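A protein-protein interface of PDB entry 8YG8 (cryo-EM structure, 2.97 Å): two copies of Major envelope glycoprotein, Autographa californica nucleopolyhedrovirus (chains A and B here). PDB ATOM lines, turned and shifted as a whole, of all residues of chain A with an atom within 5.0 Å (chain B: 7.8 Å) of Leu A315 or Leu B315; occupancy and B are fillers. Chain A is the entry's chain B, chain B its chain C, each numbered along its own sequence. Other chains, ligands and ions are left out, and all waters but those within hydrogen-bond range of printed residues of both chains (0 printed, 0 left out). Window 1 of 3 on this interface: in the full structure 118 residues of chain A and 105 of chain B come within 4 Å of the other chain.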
ATOM      1  N   MET A 311      12.483  18.093  23.081  1.00  0.00           N
ATOM      2  CA  MET A 311      11.643  19.284  23.001  1.00  0.00           C
ATOM      3  C   MET A 311      11.739  19.941  21.629  1.00  0.00           C
ATOM      4  O   MET A 311      10.722  20.351  21.055  1.00  0.00           O
ATOM      5  CB  MET A 311      12.030  20.275  24.097  1.00  0.00           C
ATOM      6  CG  MET A 311      11.131  21.494  24.169  1.00  0.00           C
ATOM      7  SD  MET A 311      11.612  22.631  25.478  1.00  0.00           S
ATOM      8  CE  MET A 311      11.107  21.707  26.924  1.00  0.00           C
ATOM      9  N   LEU A 312      12.954  20.046  21.085  1.00  0.00           N
ATOM     10  CA  LEU A 312      13.127  20.699  19.789  1.00  0.00           C
ATOM     11  C   LEU A 312      12.424  19.930  18.678  1.00  0.00           C
ATOM     12  O   LEU A 312      11.796  20.533  17.797  1.00  0.00           O
ATOM     13  CB  LEU A 312      14.615  20.854  19.474  1.00  0.00           C
ATOM     14  CG  LEU A 312      14.965  21.749  18.285  1.00  0.00           C
ATOM     15  CD1 LEU A 312      16.164  22.617  18.613  1.00  0.00           C
ATOM     16  CD2 LEU A 312      15.237  20.922  17.043  1.00  0.00           C
ATOM     17  N   HIS A 313      12.536  18.600  18.685  1.00  0.00           N
ATOM     18  CA  HIS A 313      11.858  17.824  17.648  1.00  0.00           C
ATOM     19  C   HIS A 313      10.344  17.959  17.749  1.00  0.00           C
ATOM     20  O   HIS A 313       9.655  18.080  16.725  1.00  0.00           O
ATOM     21  CB  HIS A 313      12.279  16.360  17.710  1.00  0.00           C
ATOM     22  CG  HIS A 313      13.509  16.059  16.916  1.00  0.00           C
ATOM     23  ND1 HIS A 313      14.781  16.208  17.424  1.00  0.00           N
ATOM     24  CD2 HIS A 313      13.661  15.627  15.643  1.00  0.00           C
ATOM     25  CE1 HIS A 313      15.663  15.878  16.498  1.00  0.00           C
ATOM     26  NE2 HIS A 313      15.010  15.520  15.408  1.00  0.00           N
ATOM     27  N   ASP A 314       9.804  17.948  18.971  1.00  0.00           N
ATOM     28  CA  ASP A 314       8.368  18.169  19.113  1.00  0.00           C
ATOM     29  C   ASP A 314       7.969  19.538  18.575  1.00  0.00           C
ATOM     30  O   ASP A 314       6.952  19.674  17.882  1.00  0.00           O
ATOM     31  CB  ASP A 314       7.955  18.023  20.575  1.00  0.00           C
ATOM     32  CG  ASP A 314       7.726  16.581  20.971  1.00  0.00           C
ATOM     33  OD1 ASP A 314       8.282  15.688  20.299  1.00  0.00           O
ATOM     34  OD2 ASP A 314       6.995  16.340  21.952  1.00  0.00           O
ATOM     35  N   LEU A 315       8.779  20.559  18.864  1.00  0.00           N
ATOM     36  CA  LEU A 315       8.482  21.904  18.382  1.00  0.00           C
ATOM     37  C   LEU A 315       8.438  21.951  16.861  1.00  0.00           C
ATOM     38  O   LEU A 315       7.512  22.523  16.273  1.00  0.00           O
ATOM     39  CB  LEU A 315       9.523  22.889  18.913  1.00  0.00           C
ATOM     40  CG  LEU A 315       9.640  24.217  18.163  1.00  0.00           C
ATOM     41  CD1 LEU A 315       8.413  25.072  18.395  1.00  0.00           C
ATOM     42  CD2 LEU A 315      10.898  24.960  18.575  1.00  0.00           C
ATOM     43  N   ILE A 316       9.436  21.359  16.202  1.00  0.00           N
ATOM     44  CA  ILE A 316       9.484  21.465  14.745  1.00  0.00           C
ATOM     45  C   ILE A 316       8.345  20.675  14.113  1.00  0.00           C
ATOM     46  O   ILE A 316       7.725  21.130  13.141  1.00  0.00           O
ATOM     47  CB  ILE A 316      10.857  21.034  14.190  1.00  0.00           C
ATOM     48  CG1 ILE A 316      11.138  19.557  14.452  1.00  0.00           C
ATOM     49  CG2 ILE A 316      11.964  21.887  14.783  1.00  0.00           C
ATOM     50  CD1 ILE A 316      12.352  19.040  13.719  1.00  0.00           C
ATOM     51  N   VAL A 317       8.031  19.494  14.656  1.00  0.00           N
ATOM     52  CA  VAL A 317       6.956  18.710  14.059  1.00  0.00           C
ATOM     53  C   VAL A 317       5.610  19.391  14.270  1.00  0.00           C
ATOM     54  O   VAL A 317       4.702  19.245  13.445  1.00  0.00           O
ATOM     55  CB  VAL A 317       6.959  17.266  14.596  1.00  0.00           C
ATOM     56  CG1 VAL A 317       6.387  17.198  15.999  1.00  0.00           C
ATOM     57  CG2 VAL A 317       6.180  16.358  13.660  1.00  0.00           C
ATOM     58  N   SER A 318       5.449  20.148  15.360  1.00  0.00           N
ATOM     59  CA  SER A 318       4.199  20.876  15.546  1.00  0.00           C
ATOM     60  C   SER A 318       4.117  22.087  14.626  1.00  0.00           C
ATOM     61  O   SER A 318       3.053  22.376  14.067  1.00  0.00           O
ATOM     62  CB  SER A 318       4.047  21.304  17.003  1.00  0.00           C
ATOM     63  OG  SER A 318       2.971  22.213  17.147  1.00  0.00           O
ATOM     64  N   VAL A 319       5.226  22.814  14.461  1.00  0.00           N
ATOM     65  CA  VAL A 319       5.198  24.035  13.661  1.00  0.00           C
ATOM     66  C   VAL A 319       5.040  23.726  12.177  1.00  0.00           C
ATOM     67  O   VAL A 319       4.398  24.490  11.445  1.00  0.00           O
ATOM     68  CB  VAL A 319       6.457  24.878  13.931  1.00  0.00           C
ATOM     69  CG1 VAL A 319       6.549  26.039  12.960  1.00  0.00           C
ATOM     70  CG2 VAL A 319       6.439  25.396  15.351  1.00  0.00           C
ATOM     71  N   ALA A 320       5.594  22.603  11.708  1.00  0.00           N
ATOM     72  CA  ALA A 320       5.647  22.323  10.275  1.00  0.00           C
ATOM     73  C   ALA A 320       4.291  22.364   9.580  1.00  0.00           C
ATOM     74  O   ALA A 320       4.255  22.404   8.346  1.00  0.00           O
ATOM     75  CB  ALA A 320       6.291  20.957  10.038  1.00  0.00           C
ATOM     76  N   LEU B 308      21.628  27.856  25.190  1.00  0.00           N
ATOM     77  CA  LEU B 308      20.732  27.289  24.185  1.00  0.00           C
ATOM     78  C   LEU B 308      19.316  27.132  24.722  1.00  0.00           C
ATOM     79  O   LEU B 308      18.340  27.383  24.004  1.00  0.00           O
ATOM     80  CB  LEU B 308      21.264  25.943  23.695  1.00  0.00           C
ATOM     81  CG  LEU B 308      22.038  25.971  22.379  1.00  0.00           C
ATOM     82  CD1 LEU B 308      23.381  26.655  22.560  1.00  0.00           C
ATOM     83  CD2 LEU B 308      22.214  24.562  21.844  1.00  0.00           C
ATOM     84  N   ASN B 309      19.182  26.700  25.978  1.00  0.00           N
ATOM     85  CA  ASN B 309      17.856  26.515  26.559  1.00  0.00           C
ATOM     86  C   ASN B 309      17.083  27.828  26.596  1.00  0.00           C
ATOM     87  O   ASN B 309      15.901  27.885  26.223  1.00  0.00           O
ATOM     88  CB  ASN B 309      17.985  25.927  27.964  1.00  0.00           C
ATOM     89  CG  ASN B 309      16.671  25.911  28.709  1.00  0.00           C
ATOM     90  OD1 ASN B 309      15.630  25.592  28.142  1.00  0.00           O
ATOM     91  ND2 ASN B 309      16.712  26.261  29.988  1.00  0.00           N
ATOM     92  N   ASN B 310      17.742  28.900  27.043  1.00  0.00           N
ATOM     93  CA  ASN B 310      17.066  30.193  27.099  1.00  0.00           C
ATOM     94  C   ASN B 310      16.652  30.657  25.707  1.00  0.00           C
ATOM     95  O   ASN B 310      15.530  31.156  25.515  1.00  0.00           O
ATOM     96  CB  ASN B 310      17.970  31.228  27.764  1.00  0.00           C
ATOM     97  CG  ASN B 310      18.082  31.023  29.257  1.00  0.00           C
ATOM     98  OD1 ASN B 310      17.362  30.213  29.839  1.00  0.00           O
ATOM     99  ND2 ASN B 310      18.992  31.754  29.887  1.00  0.00           N
ATOM    100  N   MET B 311      17.540  30.492  24.722  1.00  0.00           N
ATOM    101  CA  MET B 311      17.195  30.896  23.362  1.00  0.00           C
ATOM    102  C   MET B 311      15.986  30.127  22.845  1.00  0.00           C
ATOM    103  O   MET B 311      15.085  30.710  22.228  1.00  0.00           O
ATOM    104  CB  MET B 311      18.389  30.692  22.433  1.00  0.00           C
ATOM    105  CG  MET B 311      18.158  31.197  21.022  1.00  0.00           C
ATOM    106  SD  MET B 311      19.589  30.947  19.960  1.00  0.00           S
ATOM    107  CE  MET B 311      20.710  32.172  20.621  1.00  0.00           C
ATOM    108  N   LEU B 312      15.948  28.815  23.090  1.00  0.00           N
ATOM    109  CA  LEU B 312      14.833  28.004  22.608  1.00  0.00           C
ATOM    110  C   LEU B 312      13.518  28.426  23.252  1.00  0.00           C
ATOM    111  O   LEU B 312      12.477  28.479  22.582  1.00  0.00           O
ATOM    112  CB  LEU B 312      15.109  26.525  22.872  1.00  0.00           C
ATOM    113  CG  LEU B 312      14.133  25.526  22.252  1.00  0.00           C
ATOM    114  CD1 LEU B 312      14.885  24.344  21.673  1.00  0.00           C
ATOM    115  CD2 LEU B 312      13.123  25.052  23.278  1.00  0.00           C
ATOM    116  N   HIS B 313      13.538  28.709  24.557  1.00  0.00           N
ATOM    117  CA  HIS B 313      12.304  29.130  25.214  1.00  0.00           C
ATOM    118  C   HIS B 313      11.812  30.466  24.668  1.00  0.00           C
ATOM    119  O   HIS B 313      10.604  30.652  24.455  1.00  0.00           O
ATOM    120  CB  HIS B 313      12.502  29.196  26.726  1.00  0.00           C
ATOM    121  CG  HIS B 313      12.161  27.918  27.426  1.00  0.00           C
ATOM    122  ND1 HIS B 313      10.867  27.565  27.738  1.00  0.00           N
ATOM    123  CD2 HIS B 313      12.943  26.903  27.860  1.00  0.00           C
ATOM    124  CE1 HIS B 313      10.867  26.391  28.342  1.00  0.00           C
ATOM    125  NE2 HIS B 313      12.114  25.967  28.427  1.00  0.00           N
ATOM    126  N   ASP B 314      12.729  31.407  24.425  1.00  0.00           N
ATOM    127  CA  ASP B 314      12.318  32.663  23.803  1.00  0.00           C
ATOM    128  C   ASP B 314      11.700  32.416  22.432  1.00  0.00           C
ATOM    129  O   ASP B 314      10.661  32.999  22.087  1.00  0.00           O
ATOM    130  CB  ASP B 314      13.512  33.609  23.689  1.00  0.00           C
ATOM    131  CG  ASP B 314      13.817  34.318  24.989  1.00  0.00           C
ATOM    132  OD1 ASP B 314      13.510  33.755  26.060  1.00  0.00           O
ATOM    133  OD2 ASP B 314      14.363  35.440  24.942  1.00  0.00           O
ATOM    134  N   LEU B 315      12.322  31.536  21.643  1.00  0.00           N
ATOM    135  CA  LEU B 315      11.791  31.200  20.326  1.00  0.00           C
ATOM    136  C   LEU B 315      10.359  30.690  20.418  1.00  0.00           C
ATOM    137  O   LEU B 315       9.477  31.147  19.681  1.00  0.00           O
ATOM    138  CB  LEU B 315      12.681  30.154  19.658  1.00  0.00           C
ATOM    139  CG  LEU B 315      12.071  29.420  18.463  1.00  0.00           C
ATOM    140  CD1 LEU B 315      11.853  30.363  17.302  1.00  0.00           C
ATOM    141  CD2 LEU B 315      12.943  28.248  18.047  1.00  0.00           C
ATOM    142  N   ILE B 316      10.110  29.731  21.313  1.00  0.00           N
ATOM    143  CA  ILE B 316       8.788  29.113  21.343  1.00  0.00           C
ATOM    144  C   ILE B 316       7.743  30.099  21.850  1.00  0.00           C
ATOM    145  O   ILE B 316       6.618  30.147  21.333  1.00  0.00           O
ATOM    146  CB  ILE B 316       8.793  27.808  22.164  1.00  0.00           C
ATOM    147  CG1 ILE B 316       9.160  28.058  23.624  1.00  0.00           C
ATOM    148  CG2 ILE B 316       9.745  26.795  21.553  1.00  0.00           C
ATOM    149  CD1 ILE B 316       8.951  26.852  24.506  1.00  0.00           C
ATOM    150  N   VAL B 317       8.088  30.907  22.858  1.00  0.00           N
ATOM    151  CA  VAL B 317       7.093  31.844  23.370  1.00  0.00           C
ATOM    152  C   VAL B 317       6.774  32.909  22.327  1.00  0.00           C
ATOM    153  O   VAL B 317       5.647  33.414  22.276  1.00  0.00           O
ATOM    154  CB  VAL B 317       7.543  32.465  24.707  1.00  0.00           C
ATOM    155  CG1 VAL B 317       8.757  33.354  24.522  1.00  0.00           C
ATOM    156  CG2 VAL B 317       6.400  33.240  25.345  1.00  0.00           C
ATOM    157  N   SER B 318       7.739  33.263  21.472  1.00  0.00           N
ATOM    158  CA  SER B 318       7.429  34.209  20.403  1.00  0.00           C
ATOM    159  C   SER B 318       6.586  33.563  19.309  1.00  0.00           C
ATOM    160  O   SER B 318       5.654  34.186  18.789  1.00  0.00           O
ATOM    161  CB  SER B 318       8.717  34.782  19.813  1.00  0.00           C
ATOM    162  OG  SER B 318       8.446  35.496  18.620  1.00  0.00           O
ATOM    163  N   VAL B 319       6.902  32.319  18.942  1.00  0.00           N
ATOM    164  CA  VAL B 319       6.228  31.678  17.815  1.00  0.00           C
ATOM    165  C   VAL B 319       4.780  31.344  18.157  1.00  0.00           C
ATOM    166  O   VAL B 319       3.891  31.452  17.304  1.00  0.00           O
ATOM    167  CB  VAL B 319       7.008  30.427  17.369  1.00  0.00           C
ATOM    168  CG1 VAL B 319       6.157  29.555  16.463  1.00  0.00           C
ATOM    169  CG2 VAL B 319       8.280  30.832  16.655  1.00  0.00           C
ATOM    170  N   ALA B 320       4.514  30.947  19.406  1.00  0.00           N
ATOM    171  CA  ALA B 320       3.210  30.394  19.767  1.00  0.00           C
ATOM    172  C   ALA B 320       2.032  31.314  19.460  1.00  0.00           C
ATOM    173  O   ALA B 320       0.886  30.865  19.557  1.00  0.00           O
ATOM    174  CB  ALA B 320       3.195  30.038  21.254  1.00  0.00           C
ATOM    175  N   LYS B 321       2.270  32.579  19.104  1.00  0.00           N
ATOM    176  CA  LYS B 321       1.159  33.472  18.784  1.00  0.00           C
ATOM    177  C   LYS B 321       0.422  33.025  17.529  1.00  0.00           C
ATOM    178  O   LYS B 321      -0.811  33.093  17.470  1.00  0.00           O
ATOM    179  CB  LYS B 321       1.664  34.905  18.624  1.00  0.00           C
ATOM    180  CG  LYS B 321       2.586  35.362  19.734  1.00  0.00           C
ATOM    181  CD  LYS B 321       1.838  36.204  20.748  1.00  0.00           C
ATOM    182  CE  LYS B 321       2.717  36.541  21.936  1.00  0.00           C
ATOM    183  NZ  LYS B 321       4.016  37.124  21.510  1.00  0.00           N
ATOM    184  N   ASP B 323       0.748  29.803  15.797  1.00  0.00           N
ATOM    185  CA  ASP B 323       0.303  28.424  15.965  1.00  0.00           C
ATOM    186  C   ASP B 323      -0.326  28.288  17.345  1.00  0.00           C
ATOM    187  O   ASP B 323       0.375  28.315  18.361  1.00  0.00           O
ATOM    188  CB  ASP B 323       1.470  27.457  15.792  1.00  0.00           C
ATOM    189  CG  ASP B 323       1.026  26.009  15.738  1.00  0.00           C
ATOM    190  OD1 ASP B 323      -0.197  25.759  15.757  1.00  0.00           O
ATOM    191  OD2 ASP B 323       1.898  25.120  15.675  1.00  0.00           O
ATOM    192  N   LEU B 326       0.598  24.865  19.574  1.00  0.00           N
ATOM    193  CA  LEU B 326       1.978  24.506  19.883  1.00  0.00           C
ATOM    194  C   LEU B 326       2.148  24.141  21.353  1.00  0.00           C
ATOM    195  O   LEU B 326       2.816  23.153  21.680  1.00  0.00           O
ATOM    196  CB  LEU B 326       2.911  25.653  19.504  1.00  0.00           C
ATOM    197  CG  LEU B 326       4.393  25.472  19.826  1.00  0.00           C
ATOM    198  CD1 LEU B 326       4.911  24.171  19.242  1.00  0.00           C
ATOM    199  CD2 LEU B 326       5.193  26.649  19.302  1.00  0.00           C
ATOM    200  N   ASN B 329       0.683  20.729  22.080  1.00  0.00           N
ATOM    201  CA  ASN B 329       1.524  19.663  21.545  1.00  0.00           C
ATOM    202  C   ASN B 329       2.763  19.454  22.403  1.00  0.00           C
ATOM    203  O   ASN B 329       3.170  18.314  22.650  1.00  0.00           O
ATOM    204  CB  ASN B 329       1.919  19.982  20.106  1.00  0.00           C
ATOM    205  CG  ASN B 329       0.754  19.878  19.149  1.00  0.00           C
ATOM    206  OD1 ASN B 329      -0.218  19.173  19.416  1.00  0.00           O
ATOM    207  ND2 ASN B 329       0.845  20.579  18.027  1.00  0.00           N
ATOM    208  N   LEU B 330       3.380  20.543  22.865  1.00  0.00           N
ATOM    209  CA  LEU B 330       4.588  20.409  23.671  1.00  0.00           C
ATOM    210  C   LEU B 330       4.292  19.810  25.040  1.00  0.00           C
ATOM    211  O   LEU B 330       5.177  19.199  25.650  1.00  0.00           O
ATOM    212  CB  LEU B 330       5.273  21.766  23.821  1.00  0.00           C
ATOM    213  CG  LEU B 330       6.001  22.279  22.579  1.00  0.00           C
ATOM    214  CD1 LEU B 330       6.383  23.736  22.750  1.00  0.00           C
ATOM    215  CD2 LEU B 330       7.224  21.431  22.288  1.00  0.00           C
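The side-chain carboxylate (OD2) of Asp B323 sits at hydrogen-bond distance from the side-chain hydroxyl (OG) of Ser A318, 3.4 Å away.
ND2 of Asn B329 lies within hydrogen-bond range of OG of Ser A318.
Among the printed residues, merely in contact across the chains: Met A311 with Leu B312 (3.6 Å), Met A311 with Leu B330 (3.9 Å), Leu A312 with Leu B312 (3.7 Å), Asp A314 with Leu B330 (3.9 Å), Leu A315 with Leu B315 (3.9 Å), Leu A315 with Ile B316 (3.7 Å), Leu A315 with Leu B326 (3.7 Å), Leu A315 with Leu B330 (3.9 Å) and Ser A318 with Leu B326 (3.5 Å).
Of chain B, only Leu B315 (3.9 Å), Ile B316 (3.7 Å), Leu B326 (3.7 Å) and Leu B330 (3.9 Å) come within 4 Å of Leu A315.
Leu B315 touches just one residue of chain A: Leu A315 (3.9 Å).
Of the printed residues of chain A, Ile B316 touches Leu A315 (3.7 Å).
Of the printed residues of chain A, Asp B323 touches Ser A318 (3.4 Å).
Of the printed residues of chain B, Asp A314 touches Leu B330 (3.9 Å).
Of the printed residues of chain A, Asn B329 touches Ser A318.
Of the printed residues of chain B, Leu A312 touches Leu B312 (3.7 Å).
Val B319 touches none of the printed residues of chain A.
The nearest printed residue of chain B that does not touch Ser A318 is Leu B330 (5.9 Å).
Of the 10 printed residues of chain A, 5 touch a printed residue of chain B.
Met A311 touches Leu B312, but with the chains exchanged Leu A312 does not touch Met B311 (8.6 Å).
Leu A312 touches its own counterpart, Leu B312.
Leu B315 touches its own counterpart, Leu A315.
Leu A315 touches Ile B316, but with the chains exchanged Ile A316 does not touch Leu B315 (7.2 Å).
Of the 11 pairs that touch across the chains among the printed residues, 2 have their exchanged pair printed and touching as well.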
